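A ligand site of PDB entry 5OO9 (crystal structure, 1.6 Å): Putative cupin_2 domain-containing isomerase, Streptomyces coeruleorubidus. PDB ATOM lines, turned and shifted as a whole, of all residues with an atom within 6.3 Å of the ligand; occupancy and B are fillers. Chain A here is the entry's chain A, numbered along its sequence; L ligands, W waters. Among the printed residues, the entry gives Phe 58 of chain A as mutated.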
ATOM      1  N   PHE A  17      15.701  17.037  -9.866  1.00  0.00           N
ATOM      2  CA  PHE A  17      14.893  16.850 -11.069  1.00  0.00           C
ATOM      3  C   PHE A  17      15.416  15.691 -11.898  1.00  0.00           C
ATOM      4  O   PHE A  17      16.559  15.230 -11.714  1.00  0.00           O
ATOM      5  CB  PHE A  17      14.880  18.135 -11.894  1.00  0.00           C
ATOM      6  CG  PHE A  17      16.247  18.643 -12.257  1.00  0.00           C
ATOM      7  CD1 PHE A  17      16.976  19.426 -11.361  1.00  0.00           C
ATOM      8  CD2 PHE A  17      16.808  18.360 -13.496  1.00  0.00           C
ATOM      9  CE1 PHE A  17      18.233  19.891 -11.685  1.00  0.00           C
ATOM     10  CE2 PHE A  17      18.077  18.826 -13.826  1.00  0.00           C
ATOM     11  CZ  PHE A  17      18.785  19.596 -12.926  1.00  0.00           C
ATOM     12  N   LYS A  19      16.421  14.230 -15.646  1.00  0.00           N
ATOM     13  CA  LYS A  19      16.912  14.651 -16.952  1.00  0.00           C
ATOM     14  C   LYS A  19      17.327  13.422 -17.756  1.00  0.00           C
ATOM     15  O   LYS A  19      18.262  12.721 -17.390  1.00  0.00           O
ATOM     16  CB  LYS A  19      18.098  15.609 -16.801  1.00  0.00           C
ATOM     17  CG  LYS A  19      18.503  16.289 -18.095  1.00  0.00           C
ATOM     18  CD  LYS A  19      19.493  17.412 -17.846  1.00  0.00           C
ATOM     19  CE  LYS A  19      19.962  18.042 -19.142  1.00  0.00           C
ATOM     20  NZ  LYS A  19      20.878  19.184 -18.887  1.00  0.00           N
ATOM     21  N   HIS A  20      16.597  13.146 -18.832  1.00  0.00           N
ATOM     22  CA  HIS A  20      16.882  12.009 -19.724  1.00  0.00           C
ATOM     23  C   HIS A  20      17.018  10.669 -19.013  1.00  0.00           C
ATOM     24  O   HIS A  20      17.717   9.778 -19.491  1.00  0.00           O
ATOM     25  CB  HIS A  20      18.162  12.280 -20.534  1.00  0.00           C
ATOM     26  CG  HIS A  20      18.138  13.564 -21.292  1.00  0.00           C
ATOM     27  ND1 HIS A  20      17.156  13.877 -22.209  1.00  0.00           N
ATOM     28  CD2 HIS A  20      18.992  14.617 -21.292  1.00  0.00           C
ATOM     29  CE1 HIS A  20      17.397  15.064 -22.720  1.00  0.00           C
ATOM     30  NE2 HIS A  20      18.504  15.547 -22.179  1.00  0.00           N
ATOM     31  N   ILE A  22      17.992  10.266 -15.642  1.00  0.00           N
ATOM     32  CA  ILE A  22      18.753  10.338 -14.392  1.00  0.00           C
ATOM     33  C   ILE A  22      18.084  11.307 -13.433  1.00  0.00           C
ATOM     34  O   ILE A  22      17.409  12.242 -13.851  1.00  0.00           O
ATOM     35  CB  ILE A  22      20.244  10.740 -14.598  1.00  0.00           C
ATOM     36  CG1 ILE A  22      20.399  12.216 -14.976  1.00  0.00           C
ATOM     37  CG2 ILE A  22      20.884   9.826 -15.635  1.00  0.00           C
ATOM     38  CD1 ILE A  22      21.845  12.701 -14.927  1.00  0.00           C
ATOM     39  N   LEU A  24      19.011  14.058 -10.879  1.00  0.00           N
ATOM     40  CA  LEU A  24      20.070  14.977 -10.501  1.00  0.00           C
ATOM     41  C   LEU A  24      19.753  15.700  -9.209  1.00  0.00           C
ATOM     42  O   LEU A  24      18.611  16.070  -8.947  1.00  0.00           O
ATOM     43  CB  LEU A  24      20.268  16.034 -11.598  1.00  0.00           C
ATOM     44  CG  LEU A  24      21.166  15.637 -12.764  1.00  0.00           C
ATOM     45  CD1 LEU A  24      20.817  16.440 -14.009  1.00  0.00           C
ATOM     46  CD2 LEU A  24      22.628  15.830 -12.390  1.00  0.00           C
ATOM     47  N   VAL A  26      21.182  19.126  -7.685  1.00  0.00           N
ATOM     48  CA  VAL A  26      21.978  20.322  -7.892  1.00  0.00           C
ATOM     49  C   VAL A  26      21.918  21.159  -6.614  1.00  0.00           C
ATOM     50  O   VAL A  26      20.856  21.676  -6.250  1.00  0.00           O
ATOM     51  CB  VAL A  26      21.449  21.111  -9.109  1.00  0.00           C
ATOM     52  CG1 VAL A  26      22.224  22.411  -9.299  1.00  0.00           C
ATOM     53  CG2 VAL A  26      21.542  20.242 -10.368  1.00  0.00           C
ATOM     54  N   THR A  35      31.629  22.319 -10.833  1.00  0.00           N
ATOM     55  CA  THR A  35      30.290  21.977 -10.383  1.00  0.00           C
ATOM     56  C   THR A  35      30.298  20.539  -9.914  1.00  0.00           C
ATOM     57  O   THR A  35      30.697  19.647 -10.654  1.00  0.00           O
ATOM     58  CB  THR A  35      29.299  22.064 -11.552  1.00  0.00           C
ATOM     59  OG1 THR A  35      29.226  23.402 -12.043  1.00  0.00           O
ATOM     60  CG2 THR A  35      27.913  21.585 -11.143  1.00  0.00           C
ATOM     61  N   VAL A  37      27.681  17.615  -8.455  1.00  0.00           N
ATOM     62  CA  VAL A  37      26.280  17.228  -8.291  1.00  0.00           C
ATOM     63  C   VAL A  37      26.180  15.736  -7.947  1.00  0.00           C
ATOM     64  O   VAL A  37      27.141  14.987  -8.128  1.00  0.00           O
ATOM     65  CB  VAL A  37      25.464  17.508  -9.582  1.00  0.00           C
ATOM     66  CG1 VAL A  37      25.485  18.992  -9.905  1.00  0.00           C
ATOM     67  CG2 VAL A  37      25.964  16.692 -10.766  1.00  0.00           C
ATOM     68  N   VAL A  39      24.200  12.181  -8.851  1.00  0.00           N
ATOM     69  CA  VAL A  39      23.434  11.513  -9.882  1.00  0.00           C
ATOM     70  C   VAL A  39      22.947  10.163  -9.379  1.00  0.00           C
ATOM     71  O   VAL A  39      23.747   9.357  -8.887  1.00  0.00           O
ATOM     72  CB  VAL A  39      24.257  11.292 -11.164  1.00  0.00           C
ATOM     73  CG1 VAL A  39      23.471  10.490 -12.190  1.00  0.00           C
ATOM     74  CG2 VAL A  39      24.673  12.639 -11.748  1.00  0.00           C
ATOM     75  N   HIS A  45      21.018   7.146 -18.827  1.00  0.00           N
ATOM     76  CA  HIS A  45      20.896   8.494 -19.343  1.00  0.00           C
ATOM     77  C   HIS A  45      20.695   8.336 -20.842  1.00  0.00           C
ATOM     78  O   HIS A  45      21.645   8.079 -21.577  1.00  0.00           O
ATOM     79  CB  HIS A  45      22.166   9.279 -19.046  1.00  0.00           C
ATOM     80  CG  HIS A  45      22.087  10.715 -19.441  1.00  0.00           C
ATOM     81  ND1 HIS A  45      22.243  11.141 -20.741  1.00  0.00           N
ATOM     82  CD2 HIS A  45      21.846  11.825 -18.705  1.00  0.00           C
ATOM     83  CE1 HIS A  45      22.111  12.445 -20.790  1.00  0.00           C
ATOM     84  NE2 HIS A  45      21.866  12.890 -19.567  1.00  0.00           N
ATOM     85  N   GLN A  47      20.212   9.895 -23.608  1.00  0.00           N
ATOM     86  CA  GLN A  47      20.517  10.957 -24.534  1.00  0.00           C
ATOM     87  C   GLN A  47      22.029  11.011 -24.586  1.00  0.00           C
ATOM     88  O   GLN A  47      22.702  10.811 -23.564  1.00  0.00           O
ATOM     89  CB  GLN A  47      19.908  12.268 -24.057  1.00  0.00           C
ATOM     90  CG  GLN A  47      20.125  13.459 -25.003  1.00  0.00           C
ATOM     91  CD  GLN A  47      21.138  14.460 -24.489  1.00  0.00           C
ATOM     92  OE1 GLN A  47      21.743  14.279 -23.438  1.00  0.00           O
ATOM     93  NE2 GLN A  47      21.313  15.558 -25.218  1.00  0.00           N
ATOM     94  N   PHE A  49      25.292  13.347 -25.597  1.00  0.00           N
ATOM     95  CA  PHE A  49      25.667  14.732 -25.719  1.00  0.00           C
ATOM     96  C   PHE A  49      27.177  14.829 -25.595  1.00  0.00           C
ATOM     97  O   PHE A  49      27.846  13.853 -25.242  1.00  0.00           O
ATOM     98  CB  PHE A  49      25.006  15.555 -24.597  1.00  0.00           C
ATOM     99  CG  PHE A  49      25.558  15.250 -23.228  1.00  0.00           C
ATOM    100  CD1 PHE A  49      25.179  14.096 -22.550  1.00  0.00           C
ATOM    101  CD2 PHE A  49      26.498  16.091 -22.636  1.00  0.00           C
ATOM    102  CE1 PHE A  49      25.711  13.785 -21.300  1.00  0.00           C
ATOM    103  CE2 PHE A  49      27.006  15.798 -21.380  1.00  0.00           C
ATOM    104  CZ  PHE A  49      26.627  14.648 -20.716  1.00  0.00           C
ATOM    105  N   TYR A  56      33.897  15.776 -17.530  1.00  0.00           N
ATOM    106  CA  TYR A  56      32.920  15.098 -16.692  1.00  0.00           C
ATOM    107  C   TYR A  56      33.622  13.973 -15.948  1.00  0.00           C
ATOM    108  O   TYR A  56      34.154  13.056 -16.579  1.00  0.00           O
ATOM    109  CB  TYR A  56      31.817  14.499 -17.548  1.00  0.00           C
ATOM    110  CG  TYR A  56      30.631  15.390 -17.750  1.00  0.00           C
ATOM    111  CD1 TYR A  56      30.728  16.583 -18.464  1.00  0.00           C
ATOM    112  CD2 TYR A  56      29.385  15.008 -17.262  1.00  0.00           C
ATOM    113  CE1 TYR A  56      29.608  17.389 -18.654  1.00  0.00           C
ATOM    114  CE2 TYR A  56      28.282  15.799 -17.442  1.00  0.00           C
ATOM    115  CZ  TYR A  56      28.391  16.985 -18.136  1.00  0.00           C
ATOM    116  OH  TYR A  56      27.263  17.748 -18.281  1.00  0.00           O
ATOM    117  N   PHE A  58      32.947  11.103 -13.085  1.00  0.00           N
ATOM    118  CA  PHE A  58      31.975  10.361 -12.296  1.00  0.00           C
ATOM    119  C   PHE A  58      32.683   9.471 -11.289  1.00  0.00           C
ATOM    120  O   PHE A  58      33.527   8.656 -11.658  1.00  0.00           O
ATOM    121  CB  PHE A  58      31.123   9.445 -13.193  1.00  0.00           C
ATOM    122  CG  PHE A  58      30.310  10.172 -14.246  1.00  0.00           C
ATOM    123  CD1 PHE A  58      30.875  10.512 -15.475  1.00  0.00           C
ATOM    124  CD2 PHE A  58      28.959  10.425 -14.031  1.00  0.00           C
ATOM    125  CE1 PHE A  58      30.106  11.153 -16.445  1.00  0.00           C
ATOM    126  CE2 PHE A  58      28.191  11.065 -15.001  1.00  0.00           C
ATOM    127  CZ  PHE A  58      28.772  11.423 -16.209  1.00  0.00           C
ATOM    128  N   ILE A  90      28.939  11.355 -24.798  1.00  0.00           N
ATOM    129  CA  ILE A  90      28.624  10.615 -23.575  1.00  0.00           C
ATOM    130  C   ILE A  90      27.168  10.183 -23.557  1.00  0.00           C
ATOM    131  O   ILE A  90      26.270  10.999 -23.748  1.00  0.00           O
ATOM    132  CB  ILE A  90      28.813  11.469 -22.303  1.00  0.00           C
ATOM    133  CG1 ILE A  90      30.243  11.982 -22.149  1.00  0.00           C
ATOM    134  CG2 ILE A  90      28.447  10.652 -21.058  1.00  0.00           C
ATOM    135  CD1 ILE A  90      30.373  13.149 -21.188  1.00  0.00           C
ATOM    136  N   TYR A  92      25.115   6.770 -21.020  1.00  0.00           N
ATOM    137  CA  TYR A  92      25.395   5.632 -20.155  1.00  0.00           C
ATOM    138  C   TYR A  92      24.153   4.891 -19.716  1.00  0.00           C
ATOM    139  O   TYR A  92      23.038   5.419 -19.725  1.00  0.00           O
ATOM    140  CB  TYR A  92      26.224   6.065 -18.931  1.00  0.00           C
ATOM    141  CG  TYR A  92      25.713   7.250 -18.131  1.00  0.00           C
ATOM    142  CD1 TYR A  92      26.102   8.560 -18.445  1.00  0.00           C
ATOM    143  CD2 TYR A  92      24.873   7.077 -17.040  1.00  0.00           C
ATOM    144  CE1 TYR A  92      25.664   9.639 -17.701  1.00  0.00           C
ATOM    145  CE2 TYR A  92      24.431   8.148 -16.291  1.00  0.00           C
ATOM    146  CZ  TYR A  92      24.823   9.428 -16.607  1.00  0.00           C
ATOM    147  OH  TYR A  92      24.372  10.480 -15.833  1.00  0.00           O
ATOM    148  N   MET A  98      26.030   8.095  -8.010  1.00  0.00           N
ATOM    149  CA  MET A  98      27.310   8.696  -8.389  1.00  0.00           C
ATOM    150  C   MET A  98      27.457  10.116  -7.876  1.00  0.00           C
ATOM    151  O   MET A  98      26.472  10.796  -7.582  1.00  0.00           O
ATOM    152  CB  MET A  98      27.468   8.714  -9.921  1.00  0.00           C
ATOM    153  CG  MET A  98      27.267   7.370 -10.580  1.00  0.00           C
ATOM    154  SD  MET A  98      27.643   7.367 -12.352  1.00  0.00           S
ATOM    155  CE  MET A  98      26.271   8.303 -13.002  1.00  0.00           C
ATOM    156  N   LEU A 100      29.224  13.489  -9.416  1.00  0.00           N
ATOM    157  CA  LEU A 100      29.713  13.969 -10.697  1.00  0.00           C
ATOM    158  C   LEU A 100      30.323  15.355 -10.571  1.00  0.00           C
ATOM    159  O   LEU A 100      29.682  16.259 -10.045  1.00  0.00           O
ATOM    160  CB  LEU A 100      28.570  14.022 -11.712  1.00  0.00           C
ATOM    161  CG  LEU A 100      28.787  14.806 -13.008  1.00  0.00           C
ATOM    162  CD1 LEU A 100      29.937  14.249 -13.836  1.00  0.00           C
ATOM    163  CD2 LEU A 100      27.513  14.845 -13.840  1.00  0.00           C
ATOM    164  N   VAL A 102      31.788  18.439 -12.880  1.00  0.00           N
ATOM    165  CA  VAL A 102      31.931  19.088 -14.178  1.00  0.00           C
ATOM    166  C   VAL A 102      32.884  20.264 -13.980  1.00  0.00           C
ATOM    167  O   VAL A 102      32.613  21.135 -13.168  1.00  0.00           O
ATOM    168  CB  VAL A 102      30.572  19.552 -14.705  1.00  0.00           C
ATOM    169  CG1 VAL A 102      30.728  20.268 -16.050  1.00  0.00           C
ATOM    170  CG2 VAL A 102      29.616  18.368 -14.838  1.00  0.00           C
ATOM    171  N   PHE A 106      29.665  23.818 -14.797  1.00  0.00           N
ATOM    172  CA  PHE A 106      28.652  23.433 -15.776  1.00  0.00           C
ATOM    173  C   PHE A 106      27.936  24.654 -16.335  1.00  0.00           C
ATOM    174  O   PHE A 106      27.484  25.523 -15.595  1.00  0.00           O
ATOM    175  CB  PHE A 106      27.619  22.527 -15.116  1.00  0.00           C
ATOM    176  CG  PHE A 106      26.462  22.176 -16.008  1.00  0.00           C
ATOM    177  CD1 PHE A 106      26.582  21.160 -16.958  1.00  0.00           C
ATOM    178  CD2 PHE A 106      25.251  22.850 -15.905  1.00  0.00           C
ATOM    179  CE1 PHE A 106      25.518  20.845 -17.781  1.00  0.00           C
ATOM    180  CE2 PHE A 106      24.183  22.531 -16.737  1.00  0.00           C
ATOM    181  CZ  PHE A 106      24.320  21.516 -17.672  1.00  0.00           C
ATOM    182  N   GLU A 111      26.954  22.495 -23.976  1.00  0.00           N
ATOM    183  CA  GLU A 111      26.604  21.129 -24.344  1.00  0.00           C
ATOM    184  C   GLU A 111      25.867  21.076 -25.662  1.00  0.00           C
ATOM    185  O   GLU A 111      25.147  22.004 -26.030  1.00  0.00           O
ATOM    186  CB  GLU A 111      25.816  20.475 -23.206  1.00  0.00           C
ATOM    187  CG  GLU A 111      26.540  20.647 -21.881  1.00  0.00           C
ATOM    188  CD  GLU A 111      26.350  19.512 -20.890  1.00  0.00           C
ATOM    189  OE1 GLU A 111      25.251  18.934 -20.832  1.00  0.00           O
ATOM    190  OE2 GLU A 111      27.321  19.233 -20.125  1.00  0.00           O
HETATM  191  N1  LIG L   1      23.984  17.888 -15.788  1.00  0.00           N
HETATM  192  C1  LIG L   1      23.159  18.948 -15.456  1.00  0.00           C
HETATM  193  N2  LIG L   1      23.700  19.836 -14.563  1.00  0.00           N
HETATM  194  C2  LIG L   1      24.942  19.759 -13.963  1.00  0.00           C
HETATM  195  C3  LIG L   1      25.735  18.637 -14.350  1.00  0.00           C
HETATM  196  C4  LIG L   1      25.240  17.758 -15.234  1.00  0.00           C
HETATM  197  O1  LIG L   1      22.045  19.109 -15.930  1.00  0.00           O
HETATM  198  O2  LIG L   1      25.288  20.651 -13.162  1.00  0.00           O
HETATM  199  C5  LIG L   1      23.455  16.877 -16.733  1.00  0.00           C
HETATM  200  C6  LIG L   1      24.035  16.950 -18.138  1.00  0.00           C
HETATM  201  C7  LIG L   1      23.615  15.575 -18.670  1.00  0.00           C
HETATM  202  C8  LIG L   1      23.737  14.685 -17.425  1.00  0.00           C
HETATM  203  O3  LIG L   1      23.489  18.022 -18.907  1.00  0.00           O
HETATM  204  O4  LIG L   1      22.263  15.551 -19.099  1.00  0.00           O
HETATM  205  O5  LIG L   1      23.818  15.588 -16.284  1.00  0.00           O
HETATM  206  C9  LIG L   1      24.932  13.744 -17.461  1.00  0.00           C
HETATM  207  O6  LIG L   1      25.133  13.059 -16.245  1.00  0.00           O
HETATM  208  O   HOH W   1      19.911  21.097 -16.650  1.00  0.00           O
HETATM  209  O   HOH W   2      24.740  23.141 -12.221  1.00  0.00           O
HETATM  210  O   HOH W   3      21.878  16.490 -21.617  1.00  0.00           O
HETATM  211  O   HOH W   4      21.789  21.964 -13.909  1.00  0.00           O
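O3 of the ligand lies within hydrogen-bond range of OE1 of Glu 111.
An oxygen (O3) of the ligand sits at hydrogen-bond distance from the side-chain amino group (NZ) of Lys 19, at 2.9 Å.
NE2 of His 45 is in hydrogen-bond range of O4 of the ligand (2.7 Å).
OH of Tyr 92 lies within hydrogen-bond range of O6 of the ligand (2.7 Å).
The backbone carbonyl oxygen (O) of Thr 35 lies within hydrogen-bond range of the backbone NH (N) of Val 102 (2.8 Å).
ND1 of His 45 lies within hydrogen-bond range of O of Gln 47.
The backbone carbonyl oxygen (O) of Val 37 lies within hydrogen-bond range of the backbone NH (N) of Leu 100, at 2.9 Å.
The side-chain hydroxyl (OH) of Tyr 56 lies close to the side-chain carboxylate (OE1) of Glu 111 (3.5 Å).
The backbone carbonyl oxygen (O) of Tyr 92 sits at hydrogen-bond distance from the backbone NH (N) of His 45 (2.8 Å).
The backbone carbonyl oxygen of Phe 17 sits at hydrogen-bond distance from the backbone NH of Leu 24 (2.8 Å).
O of Phe 49 lies within hydrogen-bond range of N of Ile 90 (2.8 Å).
The backbone NH (N) of Phe 106 sits at hydrogen-bond distance from the side-chain hydroxyl (OG1) of Thr 35.
Residues that only touch the ligand: Tyr 56 (3.3 Å), Phe 106 (3.4 Å), Thr 35 (3.4 Å), Leu 24 (3.5 Å), Ile 22 (3.6 Å), Val 37 (3.7 Å), Phe 49 (3.8 Å), Leu 100 (3.8 Å), Phe 58 (3.9 Å) and Val 102 (3.9 Å).
Hydrophobic or aromatic side chains within 4 Å of the ligand: Ile 22, Leu 24, Val 37, His 45, Phe 49, Tyr 56, Phe 58, Tyr 92, Leu 100, Val 102 and Phe 106.
Water W3 lies within hydrogen-bond range of an oxygen (O4) of the ligand (2.7 Å) and the side-chain amide oxygen (OE1) of Gln 47 (2.9 Å).
Water W1 lies within hydrogen-bond range of O1 of the ligand (3.0 Å) and NZ of Lys 19 (3.1 Å).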
